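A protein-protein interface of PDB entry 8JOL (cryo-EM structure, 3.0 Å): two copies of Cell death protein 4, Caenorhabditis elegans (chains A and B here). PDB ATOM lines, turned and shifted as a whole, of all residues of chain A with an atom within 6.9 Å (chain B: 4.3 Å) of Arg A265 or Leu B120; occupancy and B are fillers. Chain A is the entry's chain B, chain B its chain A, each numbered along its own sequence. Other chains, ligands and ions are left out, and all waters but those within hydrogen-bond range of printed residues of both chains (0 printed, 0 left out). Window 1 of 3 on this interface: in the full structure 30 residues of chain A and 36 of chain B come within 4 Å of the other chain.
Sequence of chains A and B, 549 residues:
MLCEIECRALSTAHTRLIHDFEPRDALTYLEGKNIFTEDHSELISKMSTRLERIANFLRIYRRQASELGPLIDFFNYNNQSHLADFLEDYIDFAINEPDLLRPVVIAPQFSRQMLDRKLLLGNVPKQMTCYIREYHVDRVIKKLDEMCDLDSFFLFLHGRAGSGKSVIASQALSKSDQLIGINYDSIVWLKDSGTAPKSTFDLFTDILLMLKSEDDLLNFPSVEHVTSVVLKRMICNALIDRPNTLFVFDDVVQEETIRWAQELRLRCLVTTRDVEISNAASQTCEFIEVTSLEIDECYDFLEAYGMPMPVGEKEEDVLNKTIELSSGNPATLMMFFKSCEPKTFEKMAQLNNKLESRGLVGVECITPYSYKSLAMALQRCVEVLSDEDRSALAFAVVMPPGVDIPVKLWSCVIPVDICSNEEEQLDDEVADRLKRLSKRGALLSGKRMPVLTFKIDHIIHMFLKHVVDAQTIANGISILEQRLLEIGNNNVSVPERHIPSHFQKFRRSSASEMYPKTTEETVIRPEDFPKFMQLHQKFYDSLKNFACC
No position is printed for both chains.
Of the 11 pairs that touch across the chains among the printed residues, none has its exchanged pair printed and touching as well.
Among the printed residues, pairs that only touch across the chains: Ile A240 with Arg B117, Arg A265 with Leu B119, Arg A265 with Lys B126, Asp A151 with Asp B116, Arg A265 with Val B124, Arg A265 with Pro B125, Cys A236 with Leu B121, Cys A236 with Leu B120, Arg A233 with Leu B121 and Asn A237 with Leu B121.
Arg A265 touches just these residues of chain B: Leu B119 (3.2 Å), Leu B120 (3.1 Å), Val B124 (3.5 Å), Pro B125 (3.6 Å) and Lys B126 (3.5 Å).
Leu B120 touches two residues of chain A.
Of the printed residues of chain A, Leu B121 touches Arg A233 (3.9 Å), Cys A236 (3.8 Å) and Asn A237 (3.9 Å).
Of the printed residues of chain A, Lys B126 touches Arg A265.
Printed residues of chain B within 4 Å of Cys A236: Leu B120 and Leu B121.
Printed residues of chain A within 4 Å of Asp B116: Asp A151.
Of the printed residues of chain A, Arg B117 touches Ile A240.
The nearest residue of chain B that does not touch Arg A265 is Asp B116 (4.05 Å).
The nearest residue of chain A that does not touch Leu B120 is Leu A264 (4.1 Å).
The nearest printed residue of chain A that does not touch Lys B126 is Gln A262 (4.03 Å).
Of the 11 printed residues of chain B, 8 touch a printed residue of chain A.
Printed residues of chain B that touch a printed residue of chain A: Asp B116, Arg B117, Leu B119, Leu B120, Leu B121, Val B124, Pro B125 and Lys B126.
Hydrophobic or aromatic side chains of chain B within 4 Å of the printed part of chain A: Leu B119, Leu B120 and Leu B121.
Along chain B the printed residues that touch a printed residue of chain A span positions 116 to 126.
Among the printed residues, no Asp or Glu carboxylate lies within 4 Å of a Lys or Arg side-chain nitrogen of the other chain.
NH1 of Arg A265 sits close to N of Leu B120 (3.1 Å).
The backbone carbonyl oxygen (O) of Arg A233 sits close to the side-chain amide oxygen (OD1) of Asn A237 (2.9 Å).
ND2 of Asn B123 sits at hydrogen-bond distance from O of Leu B120 (3.5 Å).
The backbone carbonyl oxygen of Leu B119 sits at hydrogen-bond distance from the backbone NH of Val B124, 3.1 Å away.
O of Arg A233 lies within hydrogen-bond range of SG of Cys A236 (3.0 Å).
The side-chain amide oxygen (OD1) of Asn A237 is in hydrogen-bond range of the side-chain sulfur (SG) of Cys A236, at 3.3 Å.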
ATOM      1  N   ASP A 151     -23.572 -13.830  28.034  1.00  0.00           N
ATOM      2  CA  ASP A 151     -23.261 -12.606  27.292  1.00  0.00           C
ATOM      3  C   ASP A 151     -21.808 -12.542  26.804  1.00  0.00           C
ATOM      4  O   ASP A 151     -21.520 -11.882  25.797  1.00  0.00           O
ATOM      5  CB  ASP A 151     -23.585 -11.369  28.143  1.00  0.00           C
ATOM      6  CG  ASP A 151     -25.003 -11.392  28.707  1.00  0.00           C
ATOM      7  OD1 ASP A 151     -25.821 -12.231  28.261  1.00  0.00           O
ATOM      8  OD2 ASP A 151     -25.301 -10.564  29.597  1.00  0.00           O
ATOM      9  N   SER A 152     -20.913 -13.219  27.537  1.00  0.00           N
ATOM     10  CA  SER A 152     -19.465 -13.319  27.255  1.00  0.00           C
ATOM     11  C   SER A 152     -18.817 -14.360  28.184  1.00  0.00           C
ATOM     12  O   SER A 152     -19.141 -14.434  29.375  1.00  0.00           O
ATOM     13  CB  SER A 152     -18.763 -11.968  27.434  1.00  0.00           C
ATOM     14  OG  SER A 152     -18.887 -11.471  28.762  1.00  0.00           O
ATOM     15  N   PHE A 153     -17.892 -15.156  27.658  1.00  0.00           N
ATOM     16  CA  PHE A 153     -17.393 -16.313  28.415  1.00  0.00           C
ATOM     17  C   PHE A 153     -16.143 -16.938  27.780  1.00  0.00           C
ATOM     18  O   PHE A 153     -15.953 -16.853  26.557  1.00  0.00           O
ATOM     19  CB  PHE A 153     -18.486 -17.383  28.469  1.00  0.00           C
ATOM     20  CG  PHE A 153     -18.794 -17.984  27.119  1.00  0.00           C
ATOM     21  CD1 PHE A 153     -19.629 -17.335  26.231  1.00  0.00           C
ATOM     22  CD2 PHE A 153     -18.211 -19.178  26.724  1.00  0.00           C
ATOM     23  CE1 PHE A 153     -19.890 -17.879  24.994  1.00  0.00           C
ATOM     24  CE2 PHE A 153     -18.466 -19.724  25.485  1.00  0.00           C
ATOM     25  CZ  PHE A 153     -19.296 -19.078  24.623  1.00  0.00           C
ATOM     26  N   ARG A 233     -12.539   0.202  20.410  1.00  0.00           N
ATOM     27  CA  ARG A 233     -13.832   0.884  20.247  1.00  0.00           C
ATOM     28  C   ARG A 233     -14.383   0.635  18.843  1.00  0.00           C
ATOM     29  O   ARG A 233     -15.573   0.384  18.659  1.00  0.00           O
ATOM     30  CB  ARG A 233     -13.715   2.392  20.569  1.00  0.00           C
ATOM     31  CG  ARG A 233     -14.918   3.274  20.180  1.00  0.00           C
ATOM     32  CD  ARG A 233     -16.218   2.923  20.914  1.00  0.00           C
ATOM     33  NE  ARG A 233     -17.260   3.958  20.808  1.00  0.00           N
ATOM     34  CZ  ARG A 233     -17.455   4.782  19.768  1.00  0.00           C
ATOM     35  NH1 ARG A 233     -16.696   4.732  18.681  1.00  0.00           N
ATOM     36  NH2 ARG A 233     -18.439   5.674  19.814  1.00  0.00           N
ATOM     37  N   CYS A 236     -15.944  -3.077  18.768  1.00  0.00           N
ATOM     38  CA  CYS A 236     -17.214  -3.235  19.463  1.00  0.00           C
ATOM     39  C   CYS A 236     -18.324  -2.614  18.636  1.00  0.00           C
ATOM     40  O   CYS A 236     -19.439  -3.132  18.592  1.00  0.00           O
ATOM     41  CB  CYS A 236     -17.164  -2.604  20.856  1.00  0.00           C
ATOM     42  SG  CYS A 236     -17.137  -0.798  20.875  1.00  0.00           S
ATOM     43  N   ASN A 237     -18.023  -1.506  17.967  1.00  0.00           N
ATOM     44  CA  ASN A 237     -19.013  -0.893  17.098  1.00  0.00           C
ATOM     45  C   ASN A 237     -19.447  -1.911  16.064  1.00  0.00           C
ATOM     46  O   ASN A 237     -20.638  -2.159  15.889  1.00  0.00           O
ATOM     47  CB  ASN A 237     -18.439   0.346  16.414  1.00  0.00           C
ATOM     48  CG  ASN A 237     -18.033   1.421  17.403  1.00  0.00           C
ATOM     49  OD1 ASN A 237     -18.322   1.327  18.596  1.00  0.00           O
ATOM     50  ND2 ASN A 237     -17.360   2.453  16.908  1.00  0.00           N
ATOM     51  N   LEU A 239     -19.013  -5.041  16.257  1.00  0.00           N
ATOM     52  CA  LEU A 239     -19.538  -6.210  16.949  1.00  0.00           C
ATOM     53  C   LEU A 239     -21.046  -6.108  17.116  1.00  0.00           C
ATOM     54  O   LEU A 239     -21.756  -7.103  16.980  1.00  0.00           O
ATOM     55  CB  LEU A 239     -18.857  -6.368  18.310  1.00  0.00           C
ATOM     56  CG  LEU A 239     -18.935  -7.741  18.981  1.00  0.00           C
ATOM     57  CD1 LEU A 239     -20.297  -8.003  19.607  1.00  0.00           C
ATOM     58  CD2 LEU A 239     -18.552  -8.844  18.006  1.00  0.00           C
ATOM     59  N   ILE A 240     -21.542  -4.907  17.396  1.00  0.00           N
ATOM     60  CA  ILE A 240     -22.973  -4.731  17.608  1.00  0.00           C
ATOM     61  C   ILE A 240     -23.743  -5.229  16.397  1.00  0.00           C
ATOM     62  O   ILE A 240     -24.863  -5.721  16.528  1.00  0.00           O
ATOM     63  CB  ILE A 240     -23.347  -3.256  17.874  1.00  0.00           C
ATOM     64  CG1 ILE A 240     -23.522  -2.489  16.562  1.00  0.00           C
ATOM     65  CG2 ILE A 240     -22.301  -2.586  18.753  1.00  0.00           C
ATOM     66  CD1 ILE A 240     -23.800  -1.014  16.751  1.00  0.00           C
ATOM     67  N   PHE A 247     -16.054 -16.919  18.947  1.00  0.00           N
ATOM     68  CA  PHE A 247     -14.656 -16.668  18.650  1.00  0.00           C
ATOM     69  C   PHE A 247     -13.821 -17.837  19.056  1.00  0.00           C
ATOM     70  O   PHE A 247     -13.715 -18.145  20.233  1.00  0.00           O
ATOM     71  CB  PHE A 247     -14.179 -15.450  19.408  1.00  0.00           C
ATOM     72  CG  PHE A 247     -14.654 -14.160  18.823  1.00  0.00           C
ATOM     73  CD1 PHE A 247     -14.068 -13.648  17.672  1.00  0.00           C
ATOM     74  CD2 PHE A 247     -15.695 -13.453  19.414  1.00  0.00           C
ATOM     75  CE1 PHE A 247     -14.497 -12.456  17.128  1.00  0.00           C
ATOM     76  CE2 PHE A 247     -16.129 -12.259  18.874  1.00  0.00           C
ATOM     77  CZ  PHE A 247     -15.530 -11.762  17.733  1.00  0.00           C
ATOM     78  N   ARG A 259      -7.072 -10.896  28.213  1.00  0.00           N
ATOM     79  CA  ARG A 259      -7.429  -9.589  28.746  1.00  0.00           C
ATOM     80  C   ARG A 259      -8.238  -8.800  27.725  1.00  0.00           C
ATOM     81  O   ARG A 259      -9.348  -8.358  28.021  1.00  0.00           O
ATOM     82  CB  ARG A 259      -6.176  -8.821  29.166  1.00  0.00           C
ATOM     83  CG  ARG A 259      -5.319  -9.583  30.163  1.00  0.00           C
ATOM     84  CD  ARG A 259      -4.392  -8.663  30.939  1.00  0.00           C
ATOM     85  NE  ARG A 259      -3.626  -9.399  31.941  1.00  0.00           N
ATOM     86  CZ  ARG A 259      -4.053  -9.650  33.174  1.00  0.00           C
ATOM     87  NH1 ARG A 259      -5.246  -9.224  33.568  1.00  0.00           N
ATOM     88  NH2 ARG A 259      -3.287 -10.330  34.015  1.00  0.00           N
ATOM     89  N   TRP A 260      -7.698  -8.627  26.523  1.00  0.00           N
ATOM     90  CA  TRP A 260      -8.468  -7.942  25.472  1.00  0.00           C
ATOM     91  C   TRP A 260      -9.827  -8.608  25.238  1.00  0.00           C
ATOM     92  O   TRP A 260     -10.845  -7.942  25.159  1.00  0.00           O
ATOM     93  CB  TRP A 260      -7.688  -7.872  24.149  1.00  0.00           C
ATOM     94  CG  TRP A 260      -6.545  -6.872  24.128  1.00  0.00           C
ATOM     95  CD1 TRP A 260      -5.560  -6.726  25.067  1.00  0.00           C
ATOM     96  CD2 TRP A 260      -6.262  -5.905  23.108  1.00  0.00           C
ATOM     97  NE1 TRP A 260      -4.696  -5.719  24.705  1.00  0.00           N
ATOM     98  CE2 TRP A 260      -5.101  -5.205  23.507  1.00  0.00           C
ATOM     99  CE3 TRP A 260      -6.884  -5.555  21.902  1.00  0.00           C
ATOM    100  CZ2 TRP A 260      -4.552  -4.180  22.745  1.00  0.00           C
ATOM    101  CZ3 TRP A 260      -6.330  -4.536  21.144  1.00  0.00           C
ATOM    102  CH2 TRP A 260      -5.171  -3.860  21.572  1.00  0.00           C
ATOM    103  N   ALA A 261      -9.830  -9.925  25.110  1.00  0.00           N
ATOM    104  CA  ALA A 261     -11.067 -10.659  24.971  1.00  0.00           C
ATOM    105  C   ALA A 261     -12.105 -10.282  26.049  1.00  0.00           C
ATOM    106  O   ALA A 261     -13.311 -10.309  25.784  1.00  0.00           O
ATOM    107  CB  ALA A 261     -10.783 -12.146  24.990  1.00  0.00           C
ATOM    108  N   GLN A 262     -11.647  -9.921  27.248  1.00  0.00           N
ATOM    109  CA  GLN A 262     -12.559  -9.611  28.362  1.00  0.00           C
ATOM    110  C   GLN A 262     -12.923  -8.110  28.447  1.00  0.00           C
ATOM    111  O   GLN A 262     -13.875  -7.710  29.113  1.00  0.00           O
ATOM    112  CB  GLN A 262     -11.958 -10.109  29.685  1.00  0.00           C
ATOM    113  CG  GLN A 262     -12.883 -10.933  30.576  1.00  0.00           C
ATOM    114  CD  GLN A 262     -12.874 -10.444  32.021  1.00  0.00           C
ATOM    115  OE1 GLN A 262     -12.136  -9.525  32.359  1.00  0.00           O
ATOM    116  NE2 GLN A 262     -13.700 -11.047  32.873  1.00  0.00           N
ATOM    117  N   GLU A 263     -12.145  -7.275  27.778  1.00  0.00           N
ATOM    118  CA  GLU A 263     -12.497  -5.865  27.692  1.00  0.00           C
ATOM    119  C   GLU A 263     -13.527  -5.738  26.588  1.00  0.00           C
ATOM    120  O   GLU A 263     -14.375  -4.850  26.622  1.00  0.00           O
ATOM    121  CB  GLU A 263     -11.269  -4.994  27.357  1.00  0.00           C
ATOM    122  CG  GLU A 263     -10.092  -5.080  28.351  1.00  0.00           C
ATOM    123  CD  GLU A 263      -8.750  -4.687  27.726  1.00  0.00           C
ATOM    124  OE1 GLU A 263      -8.768  -4.063  26.632  1.00  0.00           O
ATOM    125  OE2 GLU A 263      -7.682  -5.009  28.325  1.00  0.00           O
ATOM    126  N   LEU A 264     -13.430  -6.632  25.603  1.00  0.00           N
ATOM    127  CA  LEU A 264     -14.298  -6.619  24.419  1.00  0.00           C
ATOM    128  C   LEU A 264     -15.531  -7.487  24.623  1.00  0.00           C
ATOM    129  O   LEU A 264     -16.257  -7.780  23.685  1.00  0.00           O
ATOM    130  CB  LEU A 264     -13.552  -7.075  23.158  1.00  0.00           C
ATOM    131  CG  LEU A 264     -12.735  -6.029  22.401  1.00  0.00           C
ATOM    132  CD1 LEU A 264     -12.630  -6.423  20.940  1.00  0.00           C
ATOM    133  CD2 LEU A 264     -13.320  -4.621  22.542  1.00  0.00           C
ATOM    134  N   ARG A 265     -15.745  -7.916  25.859  1.00  0.00           N
ATOM    135  CA  ARG A 265     -16.922  -8.704  26.202  1.00  0.00           C
ATOM    136  C   ARG A 265     -17.249  -9.782  25.158  1.00  0.00           C
ATOM    137  O   ARG A 265     -18.388  -9.926  24.726  1.00  0.00           O
ATOM    138  CB  ARG A 265     -18.096  -7.773  26.515  1.00  0.00           C
ATOM    139  CG  ARG A 265     -18.125  -7.387  27.984  1.00  0.00           C
ATOM    140  CD  ARG A 265     -18.571  -5.977  28.257  1.00  0.00           C
ATOM    141  NE  ARG A 265     -18.929  -5.840  29.670  1.00  0.00           N
ATOM    142  CZ  ARG A 265     -19.666  -4.854  30.194  1.00  0.00           C
ATOM    143  NH1 ARG A 265     -20.142  -3.878  29.417  1.00  0.00           N
ATOM    144  NH2 ARG A 265     -19.944  -4.847  31.505  1.00  0.00           N
ATOM    145  N   LEU A 266     -16.224 -10.544  24.778  1.00  0.00           N
ATOM    146  CA  LEU A 266     -16.363 -11.573  23.757  1.00  0.00           C
ATOM    147  C   LEU A 266     -16.763 -12.957  24.263  1.00  0.00           C
ATOM    148  O   LEU A 266     -16.591 -13.309  25.429  1.00  0.00           O
ATOM    149  CB  LEU A 266     -15.073 -11.695  22.953  1.00  0.00           C
ATOM    150  CG  LEU A 266     -14.620 -10.438  22.219  1.00  0.00           C
ATOM    151  CD1 LEU A 266     -13.596 -10.846  21.218  1.00  0.00           C
ATOM    152  CD2 LEU A 266     -15.772  -9.765  21.520  1.00  0.00           C
ATOM    153  N   ARG A 267     -17.305 -13.733  23.340  1.00  0.00           N
ATOM    154  CA  ARG A 267     -17.608 -15.130  23.556  1.00  0.00           C
ATOM    155  C   ARG A 267     -16.486 -15.934  22.890  1.00  0.00           C
ATOM    156  O   ARG A 267     -16.381 -15.922  21.657  1.00  0.00           O
ATOM    157  CB  ARG A 267     -18.971 -15.459  22.913  1.00  0.00           C
ATOM    158  CG  ARG A 267     -20.150 -14.608  23.443  1.00  0.00           C
ATOM    159  CD  ARG A 267     -21.401 -14.700  22.560  1.00  0.00           C
ATOM    160  NE  ARG A 267     -22.202 -13.465  22.572  1.00  0.00           N
ATOM    161  CZ  ARG A 267     -23.414 -13.336  23.124  1.00  0.00           C
ATOM    162  NH1 ARG A 267     -23.992 -14.366  23.722  1.00  0.00           N
ATOM    163  NH2 ARG A 267     -24.064 -12.174  23.077  1.00  0.00           N
ATOM    164  N   CYS A 268     -15.652 -16.604  23.697  1.00  0.00           N
ATOM    165  CA  CYS A 268     -14.411 -17.249  23.206  1.00  0.00           C
ATOM    166  C   CYS A 268     -14.231 -18.765  23.469  1.00  0.00           C
ATOM    167  O   CYS A 268     -14.292 -19.237  24.617  1.00  0.00           O
ATOM    168  CB  CYS A 268     -13.160 -16.513  23.747  1.00  0.00           C
ATOM    169  SG  CYS A 268     -13.151 -14.717  23.571  1.00  0.00           S
ATOM    170  N   ASP B 116     -26.242  -3.152  29.166  1.00  0.00           N
ATOM    171  CA  ASP B 116     -25.083  -3.847  28.637  1.00  0.00           C
ATOM    172  C   ASP B 116     -24.584  -3.258  27.301  1.00  0.00           C
ATOM    173  O   ASP B 116     -23.379  -3.048  27.132  1.00  0.00           O
ATOM    174  CB  ASP B 116     -25.372  -5.347  28.580  1.00  0.00           C
ATOM    175  CG  ASP B 116     -25.949  -5.882  29.904  1.00  0.00           C
ATOM    176  OD1 ASP B 116     -26.379  -5.064  30.759  1.00  0.00           O
ATOM    177  OD2 ASP B 116     -25.973  -7.124  30.086  1.00  0.00           O
ATOM    178  N   ARG B 117     -25.507  -2.948  26.391  1.00  0.00           N
ATOM    179  CA  ARG B 117     -25.196  -2.116  25.224  1.00  0.00           C
ATOM    180  C   ARG B 117     -24.484  -0.824  25.615  1.00  0.00           C
ATOM    181  O   ARG B 117     -23.430  -0.496  25.063  1.00  0.00           O
ATOM    182  CB  ARG B 117     -26.461  -1.793  24.418  1.00  0.00           C
ATOM    183  CG  ARG B 117     -26.738  -2.800  23.322  1.00  0.00           C
ATOM    184  CD  ARG B 117     -25.598  -3.809  23.243  1.00  0.00           C
ATOM    185  NE  ARG B 117     -25.777  -4.806  22.192  1.00  0.00           N
ATOM    186  CZ  ARG B 117     -25.177  -4.767  21.005  1.00  0.00           C
ATOM    187  NH1 ARG B 117     -24.349  -3.771  20.704  1.00  0.00           N
ATOM    188  NH2 ARG B 117     -25.401  -5.726  20.112  1.00  0.00           N
ATOM    189  N   LYS B 118     -25.055  -0.092  26.565  1.00  0.00           N
ATOM    190  CA  LYS B 118     -24.468   1.185  26.983  1.00  0.00           C
ATOM    191  C   LYS B 118     -23.140   1.006  27.747  1.00  0.00           C
ATOM    192  O   LYS B 118     -22.193   1.773  27.544  1.00  0.00           O
ATOM    193  CB  LYS B 118     -25.468   2.024  27.788  1.00  0.00           C
ATOM    194  CG  LYS B 118     -26.697   2.526  26.997  1.00  0.00           C
ATOM    195  CD  LYS B 118     -27.688   3.232  27.941  1.00  0.00           C
ATOM    196  CE  LYS B 118     -29.037   3.570  27.298  1.00  0.00           C
ATOM    197  NZ  LYS B 118     -30.105   3.861  28.316  1.00  0.00           N
ATOM    198  N   LEU B 119     -23.065  -0.008  28.612  1.00  0.00           N
ATOM    199  CA  LEU B 119     -21.823  -0.299  29.331  1.00  0.00           C
ATOM    200  C   LEU B 119     -20.725  -0.633  28.353  1.00  0.00           C
ATOM    201  O   LEU B 119     -19.654  -0.047  28.429  1.00  0.00           O
ATOM    202  CB  LEU B 119     -21.984  -1.442  30.344  1.00  0.00           C
ATOM    203  CG  LEU B 119     -22.890  -1.148  31.543  1.00  0.00           C
ATOM    204  CD1 LEU B 119     -22.716  -2.190  32.634  1.00  0.00           C
ATOM    205  CD2 LEU B 119     -22.635   0.249  32.081  1.00  0.00           C
ATOM    206  N   LEU B 120     -20.974  -1.584  27.455  1.00  0.00           N
ATOM    207  CA  LEU B 120     -19.945  -1.979  26.503  1.00  0.00           C
ATOM    208  C   LEU B 120     -19.414  -0.810  25.670  1.00  0.00           C
ATOM    209  O   LEU B 120     -18.206  -0.691  25.425  1.00  0.00           O
ATOM    210  CB  LEU B 120     -20.441  -3.075  25.561  1.00  0.00           C
ATOM    211  CG  LEU B 120     -19.370  -3.404  24.507  1.00  0.00           C
ATOM    212  CD1 LEU B 120     -18.340  -4.460  25.018  1.00  0.00           C
ATOM    213  CD2 LEU B 120     -19.987  -3.813  23.163  1.00  0.00           C
ATOM    214  N   LEU B 121     -20.317   0.045  25.219  1.00  0.00           N
ATOM    215  CA  LEU B 121     -19.915   1.117  24.318  1.00  0.00           C
ATOM    216  C   LEU B 121     -19.171   2.246  25.039  1.00  0.00           C
ATOM    217  O   LEU B 121     -18.413   3.000  24.417  1.00  0.00           O
ATOM    218  CB  LEU B 121     -21.134   1.645  23.556  1.00  0.00           C
ATOM    219  CG  LEU B 121     -21.768   0.691  22.543  1.00  0.00           C
ATOM    220  CD1 LEU B 121     -22.954   1.363  21.918  1.00  0.00           C
ATOM    221  CD2 LEU B 121     -20.773   0.263  21.465  1.00  0.00           C
ATOM    222  N   GLY B 122     -19.414   2.358  26.343  1.00  0.00           N
ATOM    223  CA  GLY B 122     -18.741   3.326  27.186  1.00  0.00           C
ATOM    224  C   GLY B 122     -17.473   2.732  27.755  1.00  0.00           C
ATOM    225  O   GLY B 122     -16.867   3.289  28.670  1.00  0.00           O
ATOM    226  N   ASN B 123     -17.083   1.579  27.214  1.00  0.00           N
ATOM    227  CA  ASN B 123     -15.847   0.878  27.597  1.00  0.00           C
ATOM    228  C   ASN B 123     -15.728   0.572  29.068  1.00  0.00           C
ATOM    229  O   ASN B 123     -14.627   0.587  29.603  1.00  0.00           O
ATOM    230  CB  ASN B 123     -14.604   1.623  27.123  1.00  0.00           C
ATOM    231  CG  ASN B 123     -14.314   1.366  25.669  1.00  0.00           C
ATOM    232  OD1 ASN B 123     -13.612   2.137  25.014  1.00  0.00           O
ATOM    233  ND2 ASN B 123     -14.873   0.273  25.143  1.00  0.00           N
ATOM    234  N   VAL B 124     -16.872   0.325  29.710  1.00  0.00           N
ATOM    235  CA  VAL B 124     -16.926  -0.146  31.093  1.00  0.00           C
ATOM    236  C   VAL B 124     -16.551  -1.623  31.164  1.00  0.00           C
ATOM    237  O   VAL B 124     -17.054  -2.444  30.388  1.00  0.00           O
ATOM    238  CB  VAL B 124     -18.324   0.074  31.726  1.00  0.00           C
ATOM    239  CG1 VAL B 124     -18.432  -0.626  33.064  1.00  0.00           C
ATOM    240  CG2 VAL B 124     -18.607   1.551  31.878  1.00  0.00           C
ATOM    241  N   PRO B 125     -15.680  -1.991  32.124  1.00  0.00           N
ATOM    242  CA  PRO B 125     -15.382  -3.419  32.261  1.00  0.00           C
ATOM    243  C   PRO B 125     -16.485  -4.156  33.004  1.00  0.00           C
ATOM    244  O   PRO B 125     -17.316  -3.518  33.648  1.00  0.00           O
ATOM    245  CB  PRO B 125     -14.094  -3.438  33.101  1.00  0.00           C
ATOM    246  CG  PRO B 125     -13.693  -2.009  33.301  1.00  0.00           C
ATOM    247  CD  PRO B 125     -14.923  -1.188  33.097  1.00  0.00           C
ATOM    248  N   LYS B 126     -16.495  -5.482  32.921  1.00  0.00           N
ATOM    249  CA  LYS B 126     -17.497  -6.266  33.631  1.00  0.00           C
ATOM    250  C   LYS B 126     -17.275  -6.180  35.131  1.00  0.00           C
ATOM    251  O   LYS B 126     -16.136  -6.168  35.595  1.00  0.00           O
ATOM    252  CB  LYS B 126     -17.453  -7.728  33.192  1.00  0.00           C
ATOM    253  CG  LYS B 126     -18.600  -8.558  33.740  1.00  0.00           C
ATOM    254  CD  LYS B 126     -18.208 -10.015  33.901  1.00  0.00           C
ATOM    255  CE  LYS B 126     -17.116 -10.172  34.946  1.00  0.00           C
ATOM    256  NZ  LYS B 126     -16.880 -11.602  35.283  1.00  0.00           N
